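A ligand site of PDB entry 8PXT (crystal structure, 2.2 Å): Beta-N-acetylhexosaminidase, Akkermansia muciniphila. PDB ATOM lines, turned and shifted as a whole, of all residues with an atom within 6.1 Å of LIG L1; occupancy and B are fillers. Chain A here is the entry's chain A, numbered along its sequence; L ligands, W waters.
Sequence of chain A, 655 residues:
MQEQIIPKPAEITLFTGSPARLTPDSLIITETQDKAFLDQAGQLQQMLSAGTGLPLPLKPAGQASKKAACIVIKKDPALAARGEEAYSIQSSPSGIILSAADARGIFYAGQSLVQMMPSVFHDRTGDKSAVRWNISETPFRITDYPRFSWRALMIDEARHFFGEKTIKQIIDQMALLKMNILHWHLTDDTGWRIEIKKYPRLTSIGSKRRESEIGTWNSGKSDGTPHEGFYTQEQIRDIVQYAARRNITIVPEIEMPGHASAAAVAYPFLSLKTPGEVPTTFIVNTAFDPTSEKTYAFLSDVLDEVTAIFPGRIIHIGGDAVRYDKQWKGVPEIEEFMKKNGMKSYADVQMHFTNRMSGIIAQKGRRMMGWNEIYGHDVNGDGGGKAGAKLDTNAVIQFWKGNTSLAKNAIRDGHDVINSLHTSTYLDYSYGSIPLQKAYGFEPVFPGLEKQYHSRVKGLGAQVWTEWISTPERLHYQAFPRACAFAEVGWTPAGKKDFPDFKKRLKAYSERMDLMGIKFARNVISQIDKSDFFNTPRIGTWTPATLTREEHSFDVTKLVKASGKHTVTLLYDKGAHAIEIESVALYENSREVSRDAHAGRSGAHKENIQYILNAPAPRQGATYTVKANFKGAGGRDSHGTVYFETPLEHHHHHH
The side-chain carboxylate of Glu 467 sits at hydrogen-bond distance from an oxygen (O3) of LIG L1, at 2.6 Å. OD2 of Asp 428 lies within hydrogen-bond range of O5 of LIG L1 (2.7 Å). OH of Tyr 426 sits at hydrogen-bond distance from O6 of LIG L1. The guanidinium group (NH2) of Arg 159 is in hydrogen-bond range of an oxygen (O2) of LIG L1 (2.9 Å). NH2 of Arg 323 sits at hydrogen-bond distance from O3 of LG2 L2, 2.8 Å away.
An oxygen (O6) of LG2 L2 is in hydrogen-bond range of an oxygen (O1) of LIG L1, 2.7 Å away.
The side-chain carboxylate of Glu 467 is in salt-bridge range of the guanidinium group of Arg 159, at 3.4 Å. NH2 of Arg 159 is in salt-bridge range of OD2 of Asp 188 (3.1 Å). NH1 of Arg 159 lies within salt-bridge range of OD2 of Asp 156, at 2.9 Å. NE1 of Trp 400 sits at hydrogen-bond distance from OE1 of Glu 373 (3.1 Å). The side-chain carboxylate (OD2) of Asp 320 lies within hydrogen-bond range of a ring nitrogen (NE2) of His 259 (2.9 Å). The side-chain carboxylate (OD1) of Asp 320 lies close to the side-chain carboxylate (OE2) of Glu 255 (2.7 Å).
Residues that only touch LIG L1: Trp 465 (3.4 Å), Trp 400 (3.5 Å), Asp 320 (3.7 Å), Tyr 429 (3.8 Å) and Trp 371 (3.9 Å). Hydrophobic or aromatic side chains within 4 Å of LIG L1: Trp 371, Trp 400, Tyr 426, Tyr 429 and Trp 465. Within 4 Å of LIG L1: Arg 159, Asp 320, Trp 371, Trp 400, Tyr 426, Asp 428, Tyr 429, Trp 465 and Glu 467. The nearest printed residue that does not touch LIG L1 is His 259 (4.01 Å).
Water W3 lies within hydrogen-bond range of the side-chain hydroxyl of Tyr 429 (2.6 Å), an oxygen (O5) of LIG L1 (2.8 Å) and an oxygen (O6) of LG2 L2 (3.1 Å). Water W1 lies within hydrogen-bond range of the side-chain carboxylate (OE2) of Glu 255 (2.8 Å), an oxygen (O2) of LIG L1 (2.9 Å), the side-chain carboxylate (OD2) of Asp 188 (3.0 Å) and a ring nitrogen (NE2) of His 259 (3.2 Å).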
ATOM      1  N   ASP A 156      -4.249 -11.974  -4.036  1.00  0.00           N
ATOM      2  CA  ASP A 156      -4.071 -11.933  -2.589  1.00  0.00           C
ATOM      3  C   ASP A 156      -3.014 -12.970  -2.211  1.00  0.00           C
ATOM      4  O   ASP A 156      -3.279 -14.173  -2.228  1.00  0.00           O
ATOM      5  CB  ASP A 156      -5.402 -12.197  -1.894  1.00  0.00           C
ATOM      6  CG  ASP A 156      -5.276 -12.359  -0.395  1.00  0.00           C
ATOM      7  OD1 ASP A 156      -4.182 -12.133   0.165  1.00  0.00           O
ATOM      8  OD2 ASP A 156      -6.292 -12.725   0.236  1.00  0.00           O
ATOM      9  N   ARG A 159      -3.322 -13.892   2.452  1.00  0.00           N
ATOM     10  CA  ARG A 159      -4.054 -15.009   3.047  1.00  0.00           C
ATOM     11  C   ARG A 159      -3.303 -16.324   2.828  1.00  0.00           C
ATOM     12  O   ARG A 159      -3.167 -17.137   3.741  1.00  0.00           O
ATOM     13  CB  ARG A 159      -5.467 -15.080   2.459  1.00  0.00           C
ATOM     14  CG  ARG A 159      -6.500 -14.237   3.203  1.00  0.00           C
ATOM     15  CD  ARG A 159      -6.022 -12.810   3.445  1.00  0.00           C
ATOM     16  NE  ARG A 159      -7.052 -11.991   4.092  1.00  0.00           N
ATOM     17  CZ  ARG A 159      -8.013 -11.342   3.441  1.00  0.00           C
ATOM     18  NH1 ARG A 159      -8.115 -11.388   2.124  1.00  0.00           N
ATOM     19  NH2 ARG A 159      -8.901 -10.637   4.139  1.00  0.00           N
ATOM     20  N   HIS A 185      -2.105  -7.587  -3.442  1.00  0.00           N
ATOM     21  CA  HIS A 185      -2.587  -7.530  -2.057  1.00  0.00           C
ATOM     22  C   HIS A 185      -1.584  -8.293  -1.201  1.00  0.00           C
ATOM     23  O   HIS A 185      -1.652  -9.520  -1.090  1.00  0.00           O
ATOM     24  CB  HIS A 185      -3.986  -8.113  -1.955  1.00  0.00           C
ATOM     25  CG  HIS A 185      -4.636  -7.909  -0.625  1.00  0.00           C
ATOM     26  ND1 HIS A 185      -5.499  -6.868  -0.365  1.00  0.00           N
ATOM     27  CD2 HIS A 185      -4.562  -8.634   0.517  1.00  0.00           C
ATOM     28  CE1 HIS A 185      -5.924  -6.948   0.882  1.00  0.00           C
ATOM     29  NE2 HIS A 185      -5.372  -8.012   1.440  1.00  0.00           N
ATOM     30  N   ASP A 188      -2.178  -8.313   5.179  1.00  0.00           N
ATOM     31  CA  ASP A 188      -3.502  -8.539   5.770  1.00  0.00           C
ATOM     32  C   ASP A 188      -3.302  -9.103   7.177  1.00  0.00           C
ATOM     33  O   ASP A 188      -2.178  -9.147   7.690  1.00  0.00           O
ATOM     34  CB  ASP A 188      -4.353  -9.469   4.891  1.00  0.00           C
ATOM     35  CG  ASP A 188      -5.842  -9.151   4.959  1.00  0.00           C
ATOM     36  OD1 ASP A 188      -6.442  -9.263   6.048  1.00  0.00           O
ATOM     37  OD2 ASP A 188      -6.411  -8.751   3.921  1.00  0.00           O
ATOM     38  N   TRP A 217     -15.294 -19.971   6.333  1.00  0.00           N
ATOM     39  CA  TRP A 217     -15.319 -19.200   7.573  1.00  0.00           C
ATOM     40  C   TRP A 217     -16.112 -19.947   8.635  1.00  0.00           C
ATOM     41  O   TRP A 217     -17.199 -20.453   8.373  1.00  0.00           O
ATOM     42  CB  TRP A 217     -15.921 -17.826   7.315  1.00  0.00           C
ATOM     43  CG  TRP A 217     -15.101 -16.960   6.385  1.00  0.00           C
ATOM     44  CD1 TRP A 217     -14.017 -16.199   6.724  1.00  0.00           C
ATOM     45  CD2 TRP A 217     -15.296 -16.764   4.979  1.00  0.00           C
ATOM     46  NE1 TRP A 217     -13.525 -15.552   5.610  1.00  0.00           N
ATOM     47  CE2 TRP A 217     -14.306 -15.883   4.533  1.00  0.00           C
ATOM     48  CE3 TRP A 217     -16.229 -17.259   4.055  1.00  0.00           C
ATOM     49  CZ2 TRP A 217     -14.207 -15.475   3.202  1.00  0.00           C
ATOM     50  CZ3 TRP A 217     -16.132 -16.854   2.735  1.00  0.00           C
ATOM     51  CH2 TRP A 217     -15.125 -15.969   2.322  1.00  0.00           C
ATOM     52  N   GLU A 255      -2.618  -2.859   3.450  1.00  0.00           N
ATOM     53  CA  GLU A 255      -3.907  -2.685   4.091  1.00  0.00           C
ATOM     54  C   GLU A 255      -3.800  -1.790   5.321  1.00  0.00           C
ATOM     55  O   GLU A 255      -2.849  -1.878   6.096  1.00  0.00           O
ATOM     56  CB  GLU A 255      -4.499  -4.044   4.491  1.00  0.00           C
ATOM     57  CG  GLU A 255      -5.582  -4.579   3.544  1.00  0.00           C
ATOM     58  CD  GLU A 255      -6.920  -3.852   3.697  1.00  0.00           C
ATOM     59  OE1 GLU A 255      -6.988  -2.819   4.405  1.00  0.00           O
ATOM     60  OE2 GLU A 255      -7.915  -4.322   3.092  1.00  0.00           O
ATOM     61  N   HIS A 259      -7.320  -4.795   8.738  1.00  0.00           N
ATOM     62  CA  HIS A 259      -6.555  -5.922   8.192  1.00  0.00           C
ATOM     63  C   HIS A 259      -5.078  -5.813   8.579  1.00  0.00           C
ATOM     64  O   HIS A 259      -4.182  -5.946   7.753  1.00  0.00           O
ATOM     65  CB  HIS A 259      -6.725  -6.000   6.675  1.00  0.00           C
ATOM     66  CG  HIS A 259      -8.110  -6.361   6.242  1.00  0.00           C
ATOM     67  ND1 HIS A 259      -8.573  -7.660   6.256  1.00  0.00           N
ATOM     68  CD2 HIS A 259      -9.137  -5.609   5.782  1.00  0.00           C
ATOM     69  CE1 HIS A 259      -9.826  -7.687   5.827  1.00  0.00           C
ATOM     70  NE2 HIS A 259     -10.184  -6.448   5.533  1.00  0.00           N
ATOM     71  N   ASP A 320     -10.854  -0.319   3.550  1.00  0.00           N
ATOM     72  CA  ASP A 320     -12.201  -0.786   3.816  1.00  0.00           C
ATOM     73  C   ASP A 320     -12.491  -0.671   5.316  1.00  0.00           C
ATOM     74  O   ASP A 320     -11.588  -0.514   6.141  1.00  0.00           O
ATOM     75  CB  ASP A 320     -12.398  -2.225   3.332  1.00  0.00           C
ATOM     76  CG  ASP A 320     -11.284  -3.150   3.792  1.00  0.00           C
ATOM     77  OD1 ASP A 320     -10.106  -2.812   3.593  1.00  0.00           O
ATOM     78  OD2 ASP A 320     -11.608  -4.218   4.355  1.00  0.00           O
ATOM     79  N   ARG A 323     -13.862  -3.121  11.695  1.00  0.00           N
ATOM     80  CA  ARG A 323     -14.936  -3.658  12.539  1.00  0.00           C
ATOM     81  C   ARG A 323     -14.970  -2.815  13.815  1.00  0.00           C
ATOM     82  O   ARG A 323     -14.328  -3.142  14.815  1.00  0.00           O
ATOM     83  CB  ARG A 323     -14.706  -5.139  12.850  1.00  0.00           C
ATOM     84  CG  ARG A 323     -14.363  -6.015  11.638  1.00  0.00           C
ATOM     85  CD  ARG A 323     -15.446  -5.973  10.562  1.00  0.00           C
ATOM     86  NE  ARG A 323     -14.902  -5.504   9.290  1.00  0.00           N
ATOM     87  CZ  ARG A 323     -15.637  -5.183   8.229  1.00  0.00           C
ATOM     88  NH1 ARG A 323     -16.960  -5.260   8.266  1.00  0.00           N
ATOM     89  NH2 ARG A 323     -15.032  -4.780   7.123  1.00  0.00           N
ATOM     90  N   TRP A 371     -10.522   1.181  -1.260  1.00  0.00           N
ATOM     91  CA  TRP A 371     -11.894   0.724  -1.354  1.00  0.00           C
ATOM     92  C   TRP A 371     -12.845   1.859  -0.989  1.00  0.00           C
ATOM     93  O   TRP A 371     -12.479   2.801  -0.280  1.00  0.00           O
ATOM     94  CB  TRP A 371     -12.117  -0.490  -0.443  1.00  0.00           C
ATOM     95  CG  TRP A 371     -11.168  -1.634  -0.728  1.00  0.00           C
ATOM     96  CD1 TRP A 371     -10.138  -2.067   0.050  1.00  0.00           C
ATOM     97  CD2 TRP A 371     -11.171  -2.471  -1.892  1.00  0.00           C
ATOM     98  NE1 TRP A 371      -9.494  -3.119  -0.553  1.00  0.00           N
ATOM     99  CE2 TRP A 371     -10.109  -3.394  -1.746  1.00  0.00           C
ATOM    100  CE3 TRP A 371     -11.957  -2.538  -3.046  1.00  0.00           C
ATOM    101  CZ2 TRP A 371      -9.815  -4.361  -2.704  1.00  0.00           C
ATOM    102  CZ3 TRP A 371     -11.672  -3.501  -3.994  1.00  0.00           C
ATOM    103  CH2 TRP A 371     -10.617  -4.402  -3.822  1.00  0.00           C
ATOM    104  N   GLU A 373     -14.913   2.850   0.951  1.00  0.00           N
ATOM    105  CA  GLU A 373     -15.137   3.449   2.267  1.00  0.00           C
ATOM    106  C   GLU A 373     -14.246   4.662   2.513  1.00  0.00           C
ATOM    107  O   GLU A 373     -14.590   5.494   3.364  1.00  0.00           O
ATOM    108  CB  GLU A 373     -14.921   2.401   3.362  1.00  0.00           C
ATOM    109  CG  GLU A 373     -15.985   1.304   3.393  1.00  0.00           C
ATOM    110  CD  GLU A 373     -15.563   0.044   2.660  1.00  0.00           C
ATOM    111  OE1 GLU A 373     -14.815   0.151   1.666  1.00  0.00           O
ATOM    112  OE2 GLU A 373     -15.961  -1.068   3.082  1.00  0.00           O
ATOM    113  N   TRP A 400     -16.468  -1.641  -4.559  1.00  0.00           N
ATOM    114  CA  TRP A 400     -16.671  -3.084  -4.417  1.00  0.00           C
ATOM    115  C   TRP A 400     -18.006  -3.472  -3.802  1.00  0.00           C
ATOM    116  O   TRP A 400     -18.384  -4.637  -3.935  1.00  0.00           O
ATOM    117  CB  TRP A 400     -15.541  -3.713  -3.591  1.00  0.00           C
ATOM    118  CG  TRP A 400     -15.544  -3.389  -2.119  1.00  0.00           C
ATOM    119  CD1 TRP A 400     -15.298  -2.187  -1.538  1.00  0.00           C
ATOM    120  CD2 TRP A 400     -15.783  -4.302  -1.039  1.00  0.00           C
ATOM    121  NE1 TRP A 400     -15.383  -2.275  -0.177  1.00  0.00           N
ATOM    122  CE2 TRP A 400     -15.681  -3.572   0.163  1.00  0.00           C
ATOM    123  CE3 TRP A 400     -16.091  -5.663  -0.972  1.00  0.00           C
ATOM    124  CZ2 TRP A 400     -15.869  -4.157   1.414  1.00  0.00           C
ATOM    125  CZ3 TRP A 400     -16.278  -6.246   0.269  1.00  0.00           C
ATOM    126  CH2 TRP A 400     -16.161  -5.493   1.447  1.00  0.00           C
ATOM    127  N   TYR A 426     -15.596 -10.916  -7.828  1.00  0.00           N
ATOM    128  CA  TYR A 426     -14.841 -11.581  -6.759  1.00  0.00           C
ATOM    129  C   TYR A 426     -14.609 -13.039  -7.133  1.00  0.00           C
ATOM    130  O   TYR A 426     -15.476 -13.898  -6.927  1.00  0.00           O
ATOM    131  CB  TYR A 426     -15.559 -11.422  -5.415  1.00  0.00           C
ATOM    132  CG  TYR A 426     -15.141 -10.157  -4.690  1.00  0.00           C
ATOM    133  CD1 TYR A 426     -14.779  -9.021  -5.410  1.00  0.00           C
ATOM    134  CD2 TYR A 426     -15.071 -10.110  -3.304  1.00  0.00           C
ATOM    135  CE1 TYR A 426     -14.373  -7.875  -4.764  1.00  0.00           C
ATOM    136  CE2 TYR A 426     -14.674  -8.958  -2.657  1.00  0.00           C
ATOM    137  CZ  TYR A 426     -14.313  -7.841  -3.391  1.00  0.00           C
ATOM    138  OH  TYR A 426     -13.914  -6.685  -2.765  1.00  0.00           O
ATOM    139  N   ASP A 428     -12.805 -15.354  -5.927  1.00  0.00           N
ATOM    140  CA  ASP A 428     -12.828 -16.390  -4.904  1.00  0.00           C
ATOM    141  C   ASP A 428     -14.205 -17.031  -4.782  1.00  0.00           C
ATOM    142  O   ASP A 428     -14.306 -18.143  -4.258  1.00  0.00           O
ATOM    143  CB  ASP A 428     -12.391 -15.839  -3.544  1.00  0.00           C
ATOM    144  CG  ASP A 428     -13.265 -14.690  -3.065  1.00  0.00           C
ATOM    145  OD1 ASP A 428     -13.509 -13.760  -3.860  1.00  0.00           O
ATOM    146  OD2 ASP A 428     -13.702 -14.728  -1.892  1.00  0.00           O
ATOM    147  N   TYR A 429     -15.252 -16.378  -5.286  1.00  0.00           N
ATOM    148  CA  TYR A 429     -16.574 -16.967  -5.260  1.00  0.00           C
ATOM    149  C   TYR A 429     -16.647 -18.151  -6.231  1.00  0.00           C
ATOM    150  O   TYR A 429     -15.854 -18.265  -7.177  1.00  0.00           O
ATOM    151  CB  TYR A 429     -17.656 -15.946  -5.654  1.00  0.00           C
ATOM    152  CG  TYR A 429     -17.832 -14.769  -4.709  1.00  0.00           C
ATOM    153  CD1 TYR A 429     -17.108 -14.654  -3.531  1.00  0.00           C
ATOM    154  CD2 TYR A 429     -18.756 -13.775  -5.001  1.00  0.00           C
ATOM    155  CE1 TYR A 429     -17.284 -13.575  -2.680  1.00  0.00           C
ATOM    156  CE2 TYR A 429     -18.945 -12.697  -4.162  1.00  0.00           C
ATOM    157  CZ  TYR A 429     -18.208 -12.596  -3.006  1.00  0.00           C
ATOM    158  OH  TYR A 429     -18.409 -11.518  -2.178  1.00  0.00           O
ATOM    159  N   TRP A 465      -9.208 -13.432  -4.019  1.00  0.00           N
ATOM    160  CA  TRP A 465      -8.921 -13.585  -2.594  1.00  0.00           C
ATOM    161  C   TRP A 465      -8.592 -15.042  -2.300  1.00  0.00           C
ATOM    162  O   TRP A 465      -9.158 -15.947  -2.918  1.00  0.00           O
ATOM    163  CB  TRP A 465     -10.126 -13.123  -1.767  1.00  0.00           C
ATOM    164  CG  TRP A 465     -10.533 -11.692  -2.043  1.00  0.00           C
ATOM    165  CD1 TRP A 465     -11.630 -11.274  -2.738  1.00  0.00           C
ATOM    166  CD2 TRP A 465      -9.840 -10.515  -1.630  1.00  0.00           C
ATOM    167  NE1 TRP A 465     -11.661  -9.897  -2.784  1.00  0.00           N
ATOM    168  CE2 TRP A 465     -10.576  -9.408  -2.115  1.00  0.00           C
ATOM    169  CE3 TRP A 465      -8.670 -10.278  -0.905  1.00  0.00           C
ATOM    170  CZ2 TRP A 465     -10.171  -8.087  -1.893  1.00  0.00           C
ATOM    171  CZ3 TRP A 465      -8.278  -8.960  -0.686  1.00  0.00           C
ATOM    172  CH2 TRP A 465      -9.024  -7.884  -1.168  1.00  0.00           C
ATOM    173  N   GLU A 467      -8.266 -16.855   0.890  1.00  0.00           N
ATOM    174  CA  GLU A 467      -8.548 -17.594   2.117  1.00  0.00           C
ATOM    175  C   GLU A 467      -8.570 -19.097   1.862  1.00  0.00           C
ATOM    176  O   GLU A 467      -7.969 -19.872   2.603  1.00  0.00           O
ATOM    177  CB  GLU A 467      -9.891 -17.158   2.720  1.00  0.00           C
ATOM    178  CG  GLU A 467      -9.867 -15.850   3.467  1.00  0.00           C
ATOM    179  CD  GLU A 467     -10.179 -14.658   2.580  1.00  0.00           C
ATOM    180  OE1 GLU A 467     -10.109 -14.796   1.341  1.00  0.00           O
ATOM    181  OE2 GLU A 467     -10.508 -13.585   3.126  1.00  0.00           O
HETATM  182  C1  LIG L   1     -14.090  -9.135   1.705  1.00  0.00           C
HETATM  183  C2  LIG L   1     -12.705  -8.745   2.207  1.00  0.00           C
HETATM  184  C3  LIG L   1     -11.598  -9.371   1.446  1.00  0.00           C
HETATM  185  C4  LIG L   1     -11.811 -10.845   1.333  1.00  0.00           C
HETATM  186  C5  LIG L   1     -13.148 -11.136   0.673  1.00  0.00           C
HETATM  187  C6  LIG L   1     -13.338 -12.608   0.500  1.00  0.00           C
HETATM  188  C7  LIG L   1     -12.693  -6.513   0.895  1.00  0.00           C
HETATM  189  C8  LIG L   1     -12.546  -4.984   0.890  1.00  0.00           C
HETATM  190  N1  LIG L   1     -12.568  -7.244   2.154  1.00  0.00           N
HETATM  191  O1  LIG L   1     -15.013  -8.748   2.626  1.00  0.00           O
HETATM  192  O2  LIG L   1     -10.333  -9.134   2.119  1.00  0.00           O
HETATM  193  O3  LIG L   1     -11.809 -11.407   2.649  1.00  0.00           O
HETATM  194  O4  LIG L   1     -14.246 -10.606   1.485  1.00  0.00           O
HETATM  195  O5  LIG L   1     -14.550 -12.822  -0.162  1.00  0.00           O
HETATM  196  O6  LIG L   1     -12.926  -7.094  -0.123  1.00  0.00           O
HETATM  197  C1  LG2 L   2     -19.233  -9.549   4.685  1.00  0.00           C
HETATM  198  C2  LG2 L   2     -19.239  -8.103   4.214  1.00  0.00           C
HETATM  199  C3  LG2 L   2     -17.965  -7.395   4.499  1.00  0.00           C
HETATM  200  C4  LG2 L   2     -17.015  -8.133   5.396  1.00  0.00           C
HETATM  201  C5  LG2 L   2     -17.601  -9.057   6.480  1.00  0.00           C
HETATM  202  C6  LG2 L   2     -17.701  -8.330   7.795  1.00  0.00           C
HETATM  203  C7  LG2 L   2     -18.625  -8.606   1.723  1.00  0.00           C
HETATM  204  C8  LG2 L   2     -19.032  -8.484   0.259  1.00  0.00           C
HETATM  205  N1  LG2 L   2     -19.529  -8.057   2.734  1.00  0.00           N
HETATM  206  O1  LG2 L   2     -20.466 -10.078   4.465  1.00  0.00           O
HETATM  207  O2  LG2 L   2     -18.294  -6.115   5.112  1.00  0.00           O
HETATM  208  O3  LG2 L   2     -16.225  -7.115   6.031  1.00  0.00           O
HETATM  209  O4  LG2 L   2     -18.915  -9.626   6.161  1.00  0.00           O
HETATM  210  O5  LG2 L   2     -18.106  -9.232   8.800  1.00  0.00           O
HETATM  211  O6  LG2 L   2     -17.593  -9.123   2.009  1.00  0.00           O
HETATM  212  O   HOH W   1      -8.547  -7.000   2.823  1.00  0.00           O
HETATM  213  O   HOH W   2     -12.444 -10.192   5.420  1.00  0.00           O
HETATM  214  O   HOH W   3     -16.659 -10.979  -0.351  1.00  0.00           O
